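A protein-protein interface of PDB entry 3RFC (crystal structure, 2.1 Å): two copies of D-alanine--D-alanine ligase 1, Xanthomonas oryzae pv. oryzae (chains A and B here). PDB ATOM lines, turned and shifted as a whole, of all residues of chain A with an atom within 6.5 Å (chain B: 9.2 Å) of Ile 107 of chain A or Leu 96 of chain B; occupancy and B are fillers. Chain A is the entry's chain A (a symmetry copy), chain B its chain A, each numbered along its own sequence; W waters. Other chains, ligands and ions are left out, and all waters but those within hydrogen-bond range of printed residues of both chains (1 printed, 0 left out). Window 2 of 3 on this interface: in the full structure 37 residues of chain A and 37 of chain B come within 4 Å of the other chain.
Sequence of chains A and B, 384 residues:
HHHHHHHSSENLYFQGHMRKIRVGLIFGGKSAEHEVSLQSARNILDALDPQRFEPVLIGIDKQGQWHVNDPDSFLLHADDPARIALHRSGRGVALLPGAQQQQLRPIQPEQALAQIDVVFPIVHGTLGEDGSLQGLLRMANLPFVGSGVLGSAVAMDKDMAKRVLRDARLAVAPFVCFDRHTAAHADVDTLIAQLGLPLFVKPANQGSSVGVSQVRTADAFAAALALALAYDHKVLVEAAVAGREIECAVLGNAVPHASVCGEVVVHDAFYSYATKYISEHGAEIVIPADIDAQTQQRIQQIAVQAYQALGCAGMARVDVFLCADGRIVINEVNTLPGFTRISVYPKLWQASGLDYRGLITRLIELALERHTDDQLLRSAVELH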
ATOM      1  N   GLY A  90      -2.755 -13.544 -23.232  1.00  0.00           N
ATOM      2  CA  GLY A  90      -1.914 -14.720 -23.230  1.00  0.00           C
ATOM      3  C   GLY A  90      -1.555 -15.162 -24.613  1.00  0.00           C
ATOM      4  O   GLY A  90      -0.908 -16.206 -24.753  1.00  0.00           O
ATOM      5  N   ARG A  91      -1.948 -14.377 -25.628  1.00  0.00           N
ATOM      6  CA  ARG A  91      -1.458 -14.524 -27.003  1.00  0.00           C
ATOM      7  C   ARG A  91      -0.017 -13.964 -27.116  1.00  0.00           C
ATOM      8  O   ARG A  91       0.189 -12.754 -27.274  1.00  0.00           O
ATOM      9  CB  ARG A  91      -2.366 -13.761 -27.986  1.00  0.00           C
ATOM     10  CG  ARG A  91      -3.814 -14.148 -27.869  1.00  0.00           C
ATOM     11  CD  ARG A  91      -4.737 -13.033 -28.334  1.00  0.00           C
ATOM     12  NE  ARG A  91      -4.487 -12.669 -29.720  1.00  0.00           N
ATOM     13  CZ  ARG A  91      -5.152 -11.710 -30.361  1.00  0.00           C
ATOM     14  NH1 ARG A  91      -6.109 -11.012 -29.732  1.00  0.00           N
ATOM     15  NH2 ARG A  91      -4.859 -11.433 -31.636  1.00  0.00           N
ATOM     16  N   GLY A  92       0.957 -14.853 -27.065  1.00  0.00           N
ATOM     17  CA  GLY A  92       2.360 -14.499 -26.946  1.00  0.00           C
ATOM     18  C   GLY A  92       2.931 -13.976 -28.233  1.00  0.00           C
ATOM     19  O   GLY A  92       2.336 -14.133 -29.311  1.00  0.00           O
ATOM     20  N   VAL A  93       4.077 -13.320 -28.115  1.00  0.00           N
ATOM     21  CA  VAL A  93       4.783 -12.711 -29.241  1.00  0.00           C
ATOM     22  C   VAL A  93       6.210 -13.192 -29.321  1.00  0.00           C
ATOM     23  O   VAL A  93       6.891 -13.154 -28.350  1.00  0.00           O
ATOM     24  CB  VAL A  93       4.908 -11.173 -29.046  1.00  0.00           C
ATOM     25  CG1 VAL A  93       5.220 -10.509 -30.343  1.00  0.00           C
ATOM     26  CG2 VAL A  93       3.625 -10.579 -28.437  1.00  0.00           C
ATOM     27  N   ALA A  94       6.674 -13.574 -30.499  1.00  0.00           N
ATOM     28  CA  ALA A  94       8.062 -13.907 -30.769  1.00  0.00           C
ATOM     29  C   ALA A  94       8.643 -12.901 -31.767  1.00  0.00           C
ATOM     30  O   ALA A  94       8.009 -12.493 -32.717  1.00  0.00           O
ATOM     31  CB  ALA A  94       8.168 -15.331 -31.385  1.00  0.00           C
ATOM     32  N   LEU A  95       9.884 -12.553 -31.536  1.00  0.00           N
ATOM     33  CA  LEU A  95      10.599 -11.669 -32.369  1.00  0.00           C
ATOM     34  C   LEU A  95      11.637 -12.457 -33.152  1.00  0.00           C
ATOM     35  O   LEU A  95      12.367 -13.307 -32.577  1.00  0.00           O
ATOM     36  CB  LEU A  95      11.277 -10.678 -31.454  1.00  0.00           C
ATOM     37  CG  LEU A  95      11.266  -9.326 -32.112  1.00  0.00           C
ATOM     38  CD1 LEU A  95      10.099  -8.522 -31.503  1.00  0.00           C
ATOM     39  CD2 LEU A  95      12.633  -8.748 -31.856  1.00  0.00           C
ATOM     40  N   ARG A 105       5.967 -12.187 -34.275  1.00  0.00           N
ATOM     41  CA  ARG A 105       5.222 -13.416 -34.539  1.00  0.00           C
ATOM     42  C   ARG A 105       4.426 -13.925 -33.399  1.00  0.00           C
ATOM     43  O   ARG A 105       4.840 -13.806 -32.264  1.00  0.00           O
ATOM     44  CB  ARG A 105       6.135 -14.525 -35.041  1.00  0.00           C
ATOM     45  CG  ARG A 105       5.873 -14.658 -36.470  1.00  0.00           C
ATOM     46  CD  ARG A 105       6.824 -15.511 -37.135  1.00  0.00           C
ATOM     47  NE  ARG A 105       7.353 -14.772 -38.271  1.00  0.00           N
ATOM     48  CZ  ARG A 105       7.874 -15.334 -39.347  1.00  0.00           C
ATOM     49  NH1 ARG A 105       7.907 -16.661 -39.421  1.00  0.00           N
ATOM     50  NH2 ARG A 105       8.388 -14.568 -40.316  1.00  0.00           N
ATOM     51  N   PRO A 106       3.252 -14.479 -33.699  1.00  0.00           N
ATOM     52  CA  PRO A 106       2.483 -15.111 -32.666  1.00  0.00           C
ATOM     53  C   PRO A 106       3.101 -16.453 -32.357  1.00  0.00           C
ATOM     54  O   PRO A 106       3.437 -17.209 -33.280  1.00  0.00           O
ATOM     55  CB  PRO A 106       1.101 -15.303 -33.321  1.00  0.00           C
ATOM     56  CG  PRO A 106       1.355 -15.277 -34.760  1.00  0.00           C
ATOM     57  CD  PRO A 106       2.500 -14.368 -34.967  1.00  0.00           C
ATOM     58  N   ILE A 107       3.304 -16.714 -31.075  1.00  0.00           N
ATOM     59  CA  ILE A 107       3.509 -18.071 -30.600  1.00  0.00           C
ATOM     60  C   ILE A 107       2.066 -18.584 -30.598  1.00  0.00           C
ATOM     61  O   ILE A 107       1.183 -17.861 -30.106  1.00  0.00           O
ATOM     62  CB  ILE A 107       4.124 -18.070 -29.180  1.00  0.00           C
ATOM     63  CG1 ILE A 107       5.017 -16.831 -28.986  1.00  0.00           C
ATOM     64  CG2 ILE A 107       4.964 -19.348 -28.950  1.00  0.00           C
ATOM     65  CD1 ILE A 107       5.411 -16.531 -27.522  1.00  0.00           C
ATOM     66  N   GLN A 108       1.802 -19.756 -31.197  1.00  0.00           N
ATOM     67  CA  GLN A 108       0.422 -20.233 -31.476  1.00  0.00           C
ATOM     68  C   GLN A 108      -0.121 -19.690 -32.799  1.00  0.00           C
ATOM     69  O   GLN A 108       0.597 -19.598 -33.793  1.00  0.00           O
ATOM     70  CB  GLN A 108      -0.570 -19.852 -30.361  1.00  0.00           C
ATOM     71  CG  GLN A 108      -0.319 -20.509 -28.986  1.00  0.00           C
ATOM     72  CD  GLN A 108      -0.572 -19.549 -27.812  1.00  0.00           C
ATOM     73  OE1 GLN A 108      -1.546 -19.699 -27.053  1.00  0.00           O
ATOM     74  NE2 GLN A 108       0.311 -18.562 -27.656  1.00  0.00           N
ATOM     75  N   GLN A 111      -1.662 -19.004 -35.512  1.00  0.00           N
ATOM     76  CA  GLN A 111      -2.135 -17.630 -35.758  1.00  0.00           C
ATOM     77  C   GLN A 111      -1.393 -16.901 -36.879  1.00  0.00           C
ATOM     78  O   GLN A 111      -0.569 -17.491 -37.594  1.00  0.00           O
ATOM     79  CB  GLN A 111      -2.039 -16.790 -34.470  1.00  0.00           C
ATOM     80  CG  GLN A 111      -2.887 -17.310 -33.345  1.00  0.00           C
ATOM     81  CD  GLN A 111      -4.173 -17.902 -33.893  1.00  0.00           C
ATOM     82  OE1 GLN A 111      -4.961 -17.199 -34.542  1.00  0.00           O
ATOM     83  NE2 GLN A 111      -4.373 -19.210 -33.678  1.00  0.00           N
ATOM     84  N   VAL B  93      16.090 -18.786 -35.418  1.00  0.00           N
ATOM     85  CA  VAL B  93      15.980 -18.485 -33.992  1.00  0.00           C
ATOM     86  C   VAL B  93      14.918 -17.447 -33.728  1.00  0.00           C
ATOM     87  O   VAL B  93      14.923 -16.439 -34.353  1.00  0.00           O
ATOM     88  CB  VAL B  93      17.290 -17.834 -33.463  1.00  0.00           C
ATOM     89  CG1 VAL B  93      17.353 -17.927 -31.978  1.00  0.00           C
ATOM     90  CG2 VAL B  93      18.534 -18.489 -34.092  1.00  0.00           C
ATOM     91  N   ALA B  94      14.056 -17.672 -32.750  1.00  0.00           N
ATOM     92  CA  ALA B  94      13.084 -16.705 -32.270  1.00  0.00           C
ATOM     93  C   ALA B  94      13.404 -16.337 -30.819  1.00  0.00           C
ATOM     94  O   ALA B  94      13.764 -17.163 -30.007  1.00  0.00           O
ATOM     95  CB  ALA B  94      11.650 -17.305 -32.323  1.00  0.00           C
ATOM     96  N   LEU B  95      13.219 -15.077 -30.518  1.00  0.00           N
ATOM     97  CA  LEU B  95      13.421 -14.560 -29.222  1.00  0.00           C
ATOM     98  C   LEU B  95      12.072 -14.248 -28.596  1.00  0.00           C
ATOM     99  O   LEU B  95      11.187 -13.634 -29.249  1.00  0.00           O
ATOM    100  CB  LEU B  95      14.225 -13.293 -29.390  1.00  0.00           C
ATOM    101  CG  LEU B  95      15.196 -13.181 -28.248  1.00  0.00           C
ATOM    102  CD1 LEU B  95      16.568 -13.674 -28.754  1.00  0.00           C
ATOM    103  CD2 LEU B  95      15.158 -11.733 -27.835  1.00  0.00           C
ATOM    104  N   LEU B  96      11.871 -14.709 -27.370  1.00  0.00           N
ATOM    105  CA  LEU B  96      10.659 -14.397 -26.625  1.00  0.00           C
ATOM    106  C   LEU B  96      10.874 -13.281 -25.616  1.00  0.00           C
ATOM    107  O   LEU B  96      11.207 -13.540 -24.476  1.00  0.00           O
ATOM    108  CB  LEU B  96      10.105 -15.638 -25.925  1.00  0.00           C
ATOM    109  CG  LEU B  96       9.950 -16.905 -26.767  1.00  0.00           C
ATOM    110  CD1 LEU B  96       8.923 -17.820 -26.133  1.00  0.00           C
ATOM    111  CD2 LEU B  96       9.539 -16.566 -28.191  1.00  0.00           C
ATOM    112  N   PRO B  97      10.696 -12.019 -26.032  1.00  0.00           N
ATOM    113  CA  PRO B  97      10.956 -10.880 -25.104  1.00  0.00           C
ATOM    114  C   PRO B  97      10.071 -10.957 -23.883  1.00  0.00           C
ATOM    115  O   PRO B  97       8.913 -11.257 -24.015  1.00  0.00           O
ATOM    116  CB  PRO B  97      10.586  -9.638 -25.935  1.00  0.00           C
ATOM    117  CG  PRO B  97       9.753 -10.146 -27.080  1.00  0.00           C
ATOM    118  CD  PRO B  97      10.239 -11.559 -27.355  1.00  0.00           C
ATOM    119  N   GLY B  98      10.631 -10.673 -22.699  1.00  0.00           N
ATOM    120  CA  GLY B  98       9.902 -10.879 -21.446  1.00  0.00           C
ATOM    121  C   GLY B  98       9.756 -12.341 -21.010  1.00  0.00           C
ATOM    122  O   GLY B  98       9.260 -12.621 -19.937  1.00  0.00           O
ATOM    123  N   ALA B  99      10.185 -13.284 -21.832  1.00  0.00           N
ATOM    124  CA  ALA B  99      10.262 -14.664 -21.358  1.00  0.00           C
ATOM    125  C   ALA B  99      11.404 -14.773 -20.344  1.00  0.00           C
ATOM    126  O   ALA B  99      12.362 -13.985 -20.367  1.00  0.00           O
ATOM    127  CB  ALA B  99      10.429 -15.651 -22.522  1.00  0.00           C
ATOM    128  N   GLN B 100      11.240 -15.712 -19.426  1.00  0.00           N
ATOM    129  CA  GLN B 100      12.142 -15.899 -18.306  1.00  0.00           C
ATOM    130  C   GLN B 100      12.951 -17.224 -18.433  1.00  0.00           C
ATOM    131  O   GLN B 100      13.989 -17.390 -17.772  1.00  0.00           O
ATOM    132  CB  GLN B 100      11.349 -15.795 -16.977  1.00  0.00           C
ATOM    133  CG  GLN B 100      12.156 -15.319 -15.742  1.00  0.00           C
ATOM    134  CD  GLN B 100      12.571 -13.844 -15.788  1.00  0.00           C
ATOM    135  OE1 GLN B 100      11.736 -12.952 -15.777  1.00  0.00           O
ATOM    136  NE2 GLN B 100      13.871 -13.597 -15.810  1.00  0.00           N
ATOM    137  N   GLN B 101      12.499 -18.141 -19.287  1.00  0.00           N
ATOM    138  CA  GLN B 101      13.294 -19.300 -19.686  1.00  0.00           C
ATOM    139  C   GLN B 101      13.018 -19.731 -21.099  1.00  0.00           C
ATOM    140  O   GLN B 101      12.057 -19.290 -21.684  1.00  0.00           O
ATOM    141  CB  GLN B 101      13.192 -20.475 -18.693  1.00  0.00           C
ATOM    142  CG  GLN B 101      11.986 -21.388 -18.846  1.00  0.00           C
ATOM    143  CD  GLN B 101      11.964 -22.389 -17.682  1.00  0.00           C
ATOM    144  OE1 GLN B 101      11.553 -22.051 -16.557  1.00  0.00           O
ATOM    145  NE2 GLN B 101      12.448 -23.604 -17.935  1.00  0.00           N
ATOM    146  N   GLN B 102      13.882 -20.553 -21.658  1.00  0.00           N
ATOM    147  CA  GLN B 102      13.786 -20.862 -23.084  1.00  0.00           C
ATOM    148  C   GLN B 102      13.541 -19.569 -23.929  1.00  0.00           C
ATOM    149  O   GLN B 102      12.761 -19.553 -24.882  1.00  0.00           O
ATOM    150  CB  GLN B 102      12.679 -21.913 -23.314  1.00  0.00           C
ATOM    151  CG  GLN B 102      13.123 -23.338 -23.020  1.00  0.00           C
ATOM    152  CD  GLN B 102      14.123 -23.834 -24.078  1.00  0.00           C
ATOM    153  OE1 GLN B 102      15.171 -24.379 -23.747  1.00  0.00           O
ATOM    154  NE2 GLN B 102      13.815 -23.598 -25.350  1.00  0.00           N
ATOM    155  N   GLN B 103      14.205 -18.485 -23.565  1.00  0.00           N
ATOM    156  CA  GLN B 103      13.978 -17.206 -24.249  1.00  0.00           C
ATOM    157  C   GLN B 103      14.322 -17.245 -25.718  1.00  0.00           C
ATOM    158  O   GLN B 103      13.685 -16.568 -26.525  1.00  0.00           O
ATOM    159  CB  GLN B 103      14.728 -16.081 -23.579  1.00  0.00           C
ATOM    160  CG  GLN B 103      14.486 -16.037 -22.154  1.00  0.00           C
ATOM    161  CD  GLN B 103      15.533 -16.806 -21.451  1.00  0.00           C
ATOM    162  OE1 GLN B 103      15.804 -17.965 -21.788  1.00  0.00           O
ATOM    163  NE2 GLN B 103      16.160 -16.177 -20.465  1.00  0.00           N
ATOM    164  N   LEU B 104      15.306 -18.091 -26.047  1.00  0.00           N
ATOM    165  CA  LEU B 104      15.727 -18.348 -27.399  1.00  0.00           C
ATOM    166  C   LEU B 104      15.113 -19.610 -27.967  1.00  0.00           C
ATOM    167  O   LEU B 104      15.182 -20.691 -27.388  1.00  0.00           O
ATOM    168  CB  LEU B 104      17.245 -18.398 -27.461  1.00  0.00           C
ATOM    169  CG  LEU B 104      17.758 -16.980 -27.676  1.00  0.00           C
ATOM    170  CD1 LEU B 104      17.518 -16.182 -26.430  1.00  0.00           C
ATOM    171  CD2 LEU B 104      19.206 -16.888 -28.053  1.00  0.00           C
ATOM    172  N   ARG B 105      14.487 -19.481 -29.113  1.00  0.00           N
ATOM    173  CA  ARG B 105      13.693 -20.597 -29.625  1.00  0.00           C
ATOM    174  C   ARG B 105      13.932 -20.938 -31.045  1.00  0.00           C
ATOM    175  O   ARG B 105      14.170 -20.062 -31.852  1.00  0.00           O
ATOM    176  CB  ARG B 105      12.205 -20.366 -29.413  1.00  0.00           C
ATOM    177  CG  ARG B 105      11.804 -21.243 -28.318  1.00  0.00           C
ATOM    178  CD  ARG B 105      10.470 -20.973 -27.846  1.00  0.00           C
ATOM    179  NE  ARG B 105      10.547 -20.789 -26.403  1.00  0.00           N
ATOM    180  CZ  ARG B 105       9.535 -20.975 -25.576  1.00  0.00           C
ATOM    181  NH1 ARG B 105       8.369 -21.376 -26.071  1.00  0.00           N
ATOM    182  NH2 ARG B 105       9.689 -20.723 -24.271  1.00  0.00           N
ATOM    183  N   PRO B 106      13.893 -22.233 -31.356  1.00  0.00           N
ATOM    184  CA  PRO B 106      13.984 -22.634 -32.731  1.00  0.00           C
ATOM    185  C   PRO B 106      12.656 -22.376 -33.397  1.00  0.00           C
ATOM    186  O   PRO B 106      11.603 -22.712 -32.836  1.00  0.00           O
ATOM    187  CB  PRO B 106      14.246 -24.151 -32.640  1.00  0.00           C
ATOM    188  CG  PRO B 106      13.750 -24.543 -31.323  1.00  0.00           C
ATOM    189  CD  PRO B 106      13.962 -23.385 -30.433  1.00  0.00           C
ATOM    190  N   ILE B 107      12.705 -21.730 -34.553  1.00  0.00           N
ATOM    191  CA  ILE B 107      11.591 -21.758 -35.486  1.00  0.00           C
ATOM    192  C   ILE B 107      11.792 -23.141 -36.113  1.00  0.00           C
ATOM    193  O   ILE B 107      12.935 -23.465 -36.475  1.00  0.00           O
ATOM    194  CB  ILE B 107      11.721 -20.624 -36.531  1.00  0.00           C
ATOM    195  CG1 ILE B 107      12.438 -19.409 -35.913  1.00  0.00           C
ATOM    196  CG2 ILE B 107      10.327 -20.191 -37.040  1.00  0.00           C
ATOM    197  CD1 ILE B 107      12.932 -18.355 -36.930  1.00  0.00           C
ATOM    198  N   LEU B 136      18.437  -6.232 -27.001  1.00  0.00           N
ATOM    199  CA  LEU B 136      17.682  -7.453 -27.261  1.00  0.00           C
ATOM    200  C   LEU B 136      17.946  -8.497 -26.160  1.00  0.00           C
ATOM    201  O   LEU B 136      17.030  -9.172 -25.736  1.00  0.00           O
ATOM    202  CB  LEU B 136      18.054  -8.036 -28.646  1.00  0.00           C
ATOM    203  CG  LEU B 136      17.497  -9.445 -28.971  1.00  0.00           C
ATOM    204  CD1 LEU B 136      17.704  -9.858 -30.408  1.00  0.00           C
ATOM    205  CD2 LEU B 136      18.247 -10.573 -28.094  1.00  0.00           C
ATOM    206  N   LEU B 137      19.174  -8.612 -25.690  1.00  0.00           N
ATOM    207  CA  LEU B 137      19.547  -9.611 -24.736  1.00  0.00           C
ATOM    208  C   LEU B 137      18.949  -9.282 -23.374  1.00  0.00           C
ATOM    209  O   LEU B 137      18.420 -10.176 -22.726  1.00  0.00           O
ATOM    210  CB  LEU B 137      21.070  -9.745 -24.648  1.00  0.00           C
ATOM    211  CG  LEU B 137      21.684 -10.431 -25.896  1.00  0.00           C
ATOM    212  CD1 LEU B 137      23.162 -10.409 -25.762  1.00  0.00           C
ATOM    213  CD2 LEU B 137      21.267 -11.925 -26.046  1.00  0.00           C
ATOM    214  N   ARG B 138      19.030  -8.018 -22.936  1.00  0.00           N
ATOM    215  CA  ARG B 138      18.206  -7.515 -21.818  1.00  0.00           C
ATOM    216  C   ARG B 138      16.730  -7.774 -21.909  1.00  0.00           C
ATOM    217  O   ARG B 138      16.055  -8.063 -20.898  1.00  0.00           O
ATOM    218  CB  ARG B 138      18.402  -6.001 -21.636  1.00  0.00           C
ATOM    219  CG  ARG B 138      19.778  -5.741 -21.076  1.00  0.00           C
ATOM    220  CD  ARG B 138      20.088  -4.299 -20.894  1.00  0.00           C
ATOM    221  NE  ARG B 138      19.100  -3.550 -20.088  1.00  0.00           N
ATOM    222  CZ  ARG B 138      19.070  -3.437 -18.767  1.00  0.00           C
ATOM    223  NH1 ARG B 138      19.954  -4.041 -17.998  1.00  0.00           N
ATOM    224  NH2 ARG B 138      18.123  -2.704 -18.210  1.00  0.00           N
ATOM    225  N   MET B 139      16.185  -7.609 -23.110  1.00  0.00           N
ATOM    226  CA  MET B 139      14.711  -7.759 -23.251  1.00  0.00           C
ATOM    227  C   MET B 139      14.328  -9.221 -23.105  1.00  0.00           C
ATOM    228  O   MET B 139      13.175  -9.537 -22.764  1.00  0.00           O
ATOM    229  CB  MET B 139      14.229  -7.278 -24.613  1.00  0.00           C
ATOM    230  CG  MET B 139      14.299  -5.766 -24.789  1.00  0.00           C
ATOM    231  SD  MET B 139      13.328  -4.781 -23.611  1.00  0.00           S
ATOM    232  CE  MET B 139      11.643  -5.497 -23.777  1.00  0.00           C
ATOM    233  N   ALA B 140      15.308 -10.100 -23.359  1.00  0.00           N
ATOM    234  CA  ALA B 140      15.130 -11.496 -23.176  1.00  0.00           C
ATOM    235  C   ALA B 140      15.603 -11.959 -21.788  1.00  0.00           C
ATOM    236  O   ALA B 140      15.678 -13.139 -21.536  1.00  0.00           O
ATOM    237  CB  ALA B 140      15.893 -12.241 -24.257  1.00  0.00           C
ATOM    238  N   ASN B 141      15.934 -11.040 -20.909  1.00  0.00           N
ATOM    239  CA  ASN B 141      16.390 -11.368 -19.573  1.00  0.00           C
ATOM    240  C   ASN B 141      17.610 -12.312 -19.602  1.00  0.00           C
ATOM    241  O   ASN B 141      17.724 -13.218 -18.752  1.00  0.00           O
ATOM    242  CB  ASN B 141      15.235 -12.051 -18.811  1.00  0.00           C
ATOM    243  CG  ASN B 141      14.118 -11.104 -18.490  1.00  0.00           C
ATOM    244  OD1 ASN B 141      14.356 -10.109 -17.839  1.00  0.00           O
ATOM    245  ND2 ASN B 141      12.883 -11.396 -18.969  1.00  0.00           N
ATOM    246  N   LEU B 142      18.481 -12.157 -20.595  1.00  0.00           N
ATOM    247  CA  LEU B 142      19.682 -13.017 -20.660  1.00  0.00           C
ATOM    248  C   LEU B 142      20.936 -12.346 -20.132  1.00  0.00           C
ATOM    249  O   LEU B 142      21.314 -11.254 -20.606  1.00  0.00           O
ATOM    250  CB  LEU B 142      19.894 -13.474 -22.096  1.00  0.00           C
ATOM    251  CG  LEU B 142      18.938 -14.557 -22.585  1.00  0.00           C
ATOM    252  CD1 LEU B 142      18.946 -14.627 -24.102  1.00  0.00           C
ATOM    253  CD2 LEU B 142      19.233 -15.936 -22.003  1.00  0.00           C
HETATM  254  O   HOH W   1       7.463 -13.452 -25.758  1.00  0.00           O
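Ala 94 of chain A touches Leu 95 of chain B, and with the chains exchanged Leu 95 of chain A touches Ala 94 of chain B. Leu 95 of chain A touches its own counterpart, Leu 95 of chain B. Positions printed for both chains: 93, 94, 95, 105, 106 and 107. Of the 6 pairs that touch across the chains among the printed residues, 3 have their exchanged pair printed and touching as well.
N of Ala 94 of chain B is in hydrogen-bond range of O of Arg 105 of chain B. N of Ala 94 of chain A lies within hydrogen-bond range of O of Arg 105 of chain A (2.6 Å). N of Leu 96 of chain B lies within hydrogen-bond range of O of Gln 103 of chain B (2.7 Å). O of Gly 92 of chain A is in hydrogen-bond range of N of Ile 107 of chain A.
O of Leu 95 of chain A sits at hydrogen-bond distance from N of Leu 95 of chain B, 2.8 Å away.
Water W1 bridges O of Val 93 of chain A (2.7 Å) and O of Pro 97 of chain B (3.2 Å).
Of the printed residues of chain B, Ile 107 of chain A touches Leu 96. Of the printed residues of chain A, Leu 96 of chain B touches Ala 94 and Ile 107. Pro 106 of chain A touches none of the printed residues of chain B. Printed residues of chain B within 4 Å of Ala 94 of chain A: Leu 95 (3.5 Å) and Leu 96 (3.7 Å). Of the printed residues of chain B, Val 93 of chain A touches Pro 97 (3.8 Å). Of the printed residues of chain A, Pro 97 of chain B touches Val 93 (3.8 Å). Printed residues of chain A within 4 Å of Leu 95 of chain B: Ala 94 and Leu 95. The nearest printed residue of chain B that does not touch Ile 107 of chain A is Arg 105 of chain B (4.9 Å). The nearest printed residue of chain A that does not touch Leu 96 of chain B is Val 93 of chain A (4.3 Å).
Printed residues of chain A that touch a printed residue of chain B: Val 93, Ala 94, Leu 95 and Ile 107. Along chain A the printed residues that touch a printed residue of chain B span positions 93 to 107. Among the printed residues, 6 pairs touch across the chains. Among the printed residues, no Asp or Glu carboxylate lies within 4 Å of a Lys or Arg side-chain nitrogen of the other chain.
Among the printed residues, merely in contact across the chains: Ala 94 of chain A with Leu 95 of chain B, Leu 95 of chain A with Ala 94 of chain B, Ala 94 of chain A with Leu 96 of chain B, Val 93 of chain A with Pro 97 of chain B and Ile 107 of chain A with Leu 96 of chain B.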
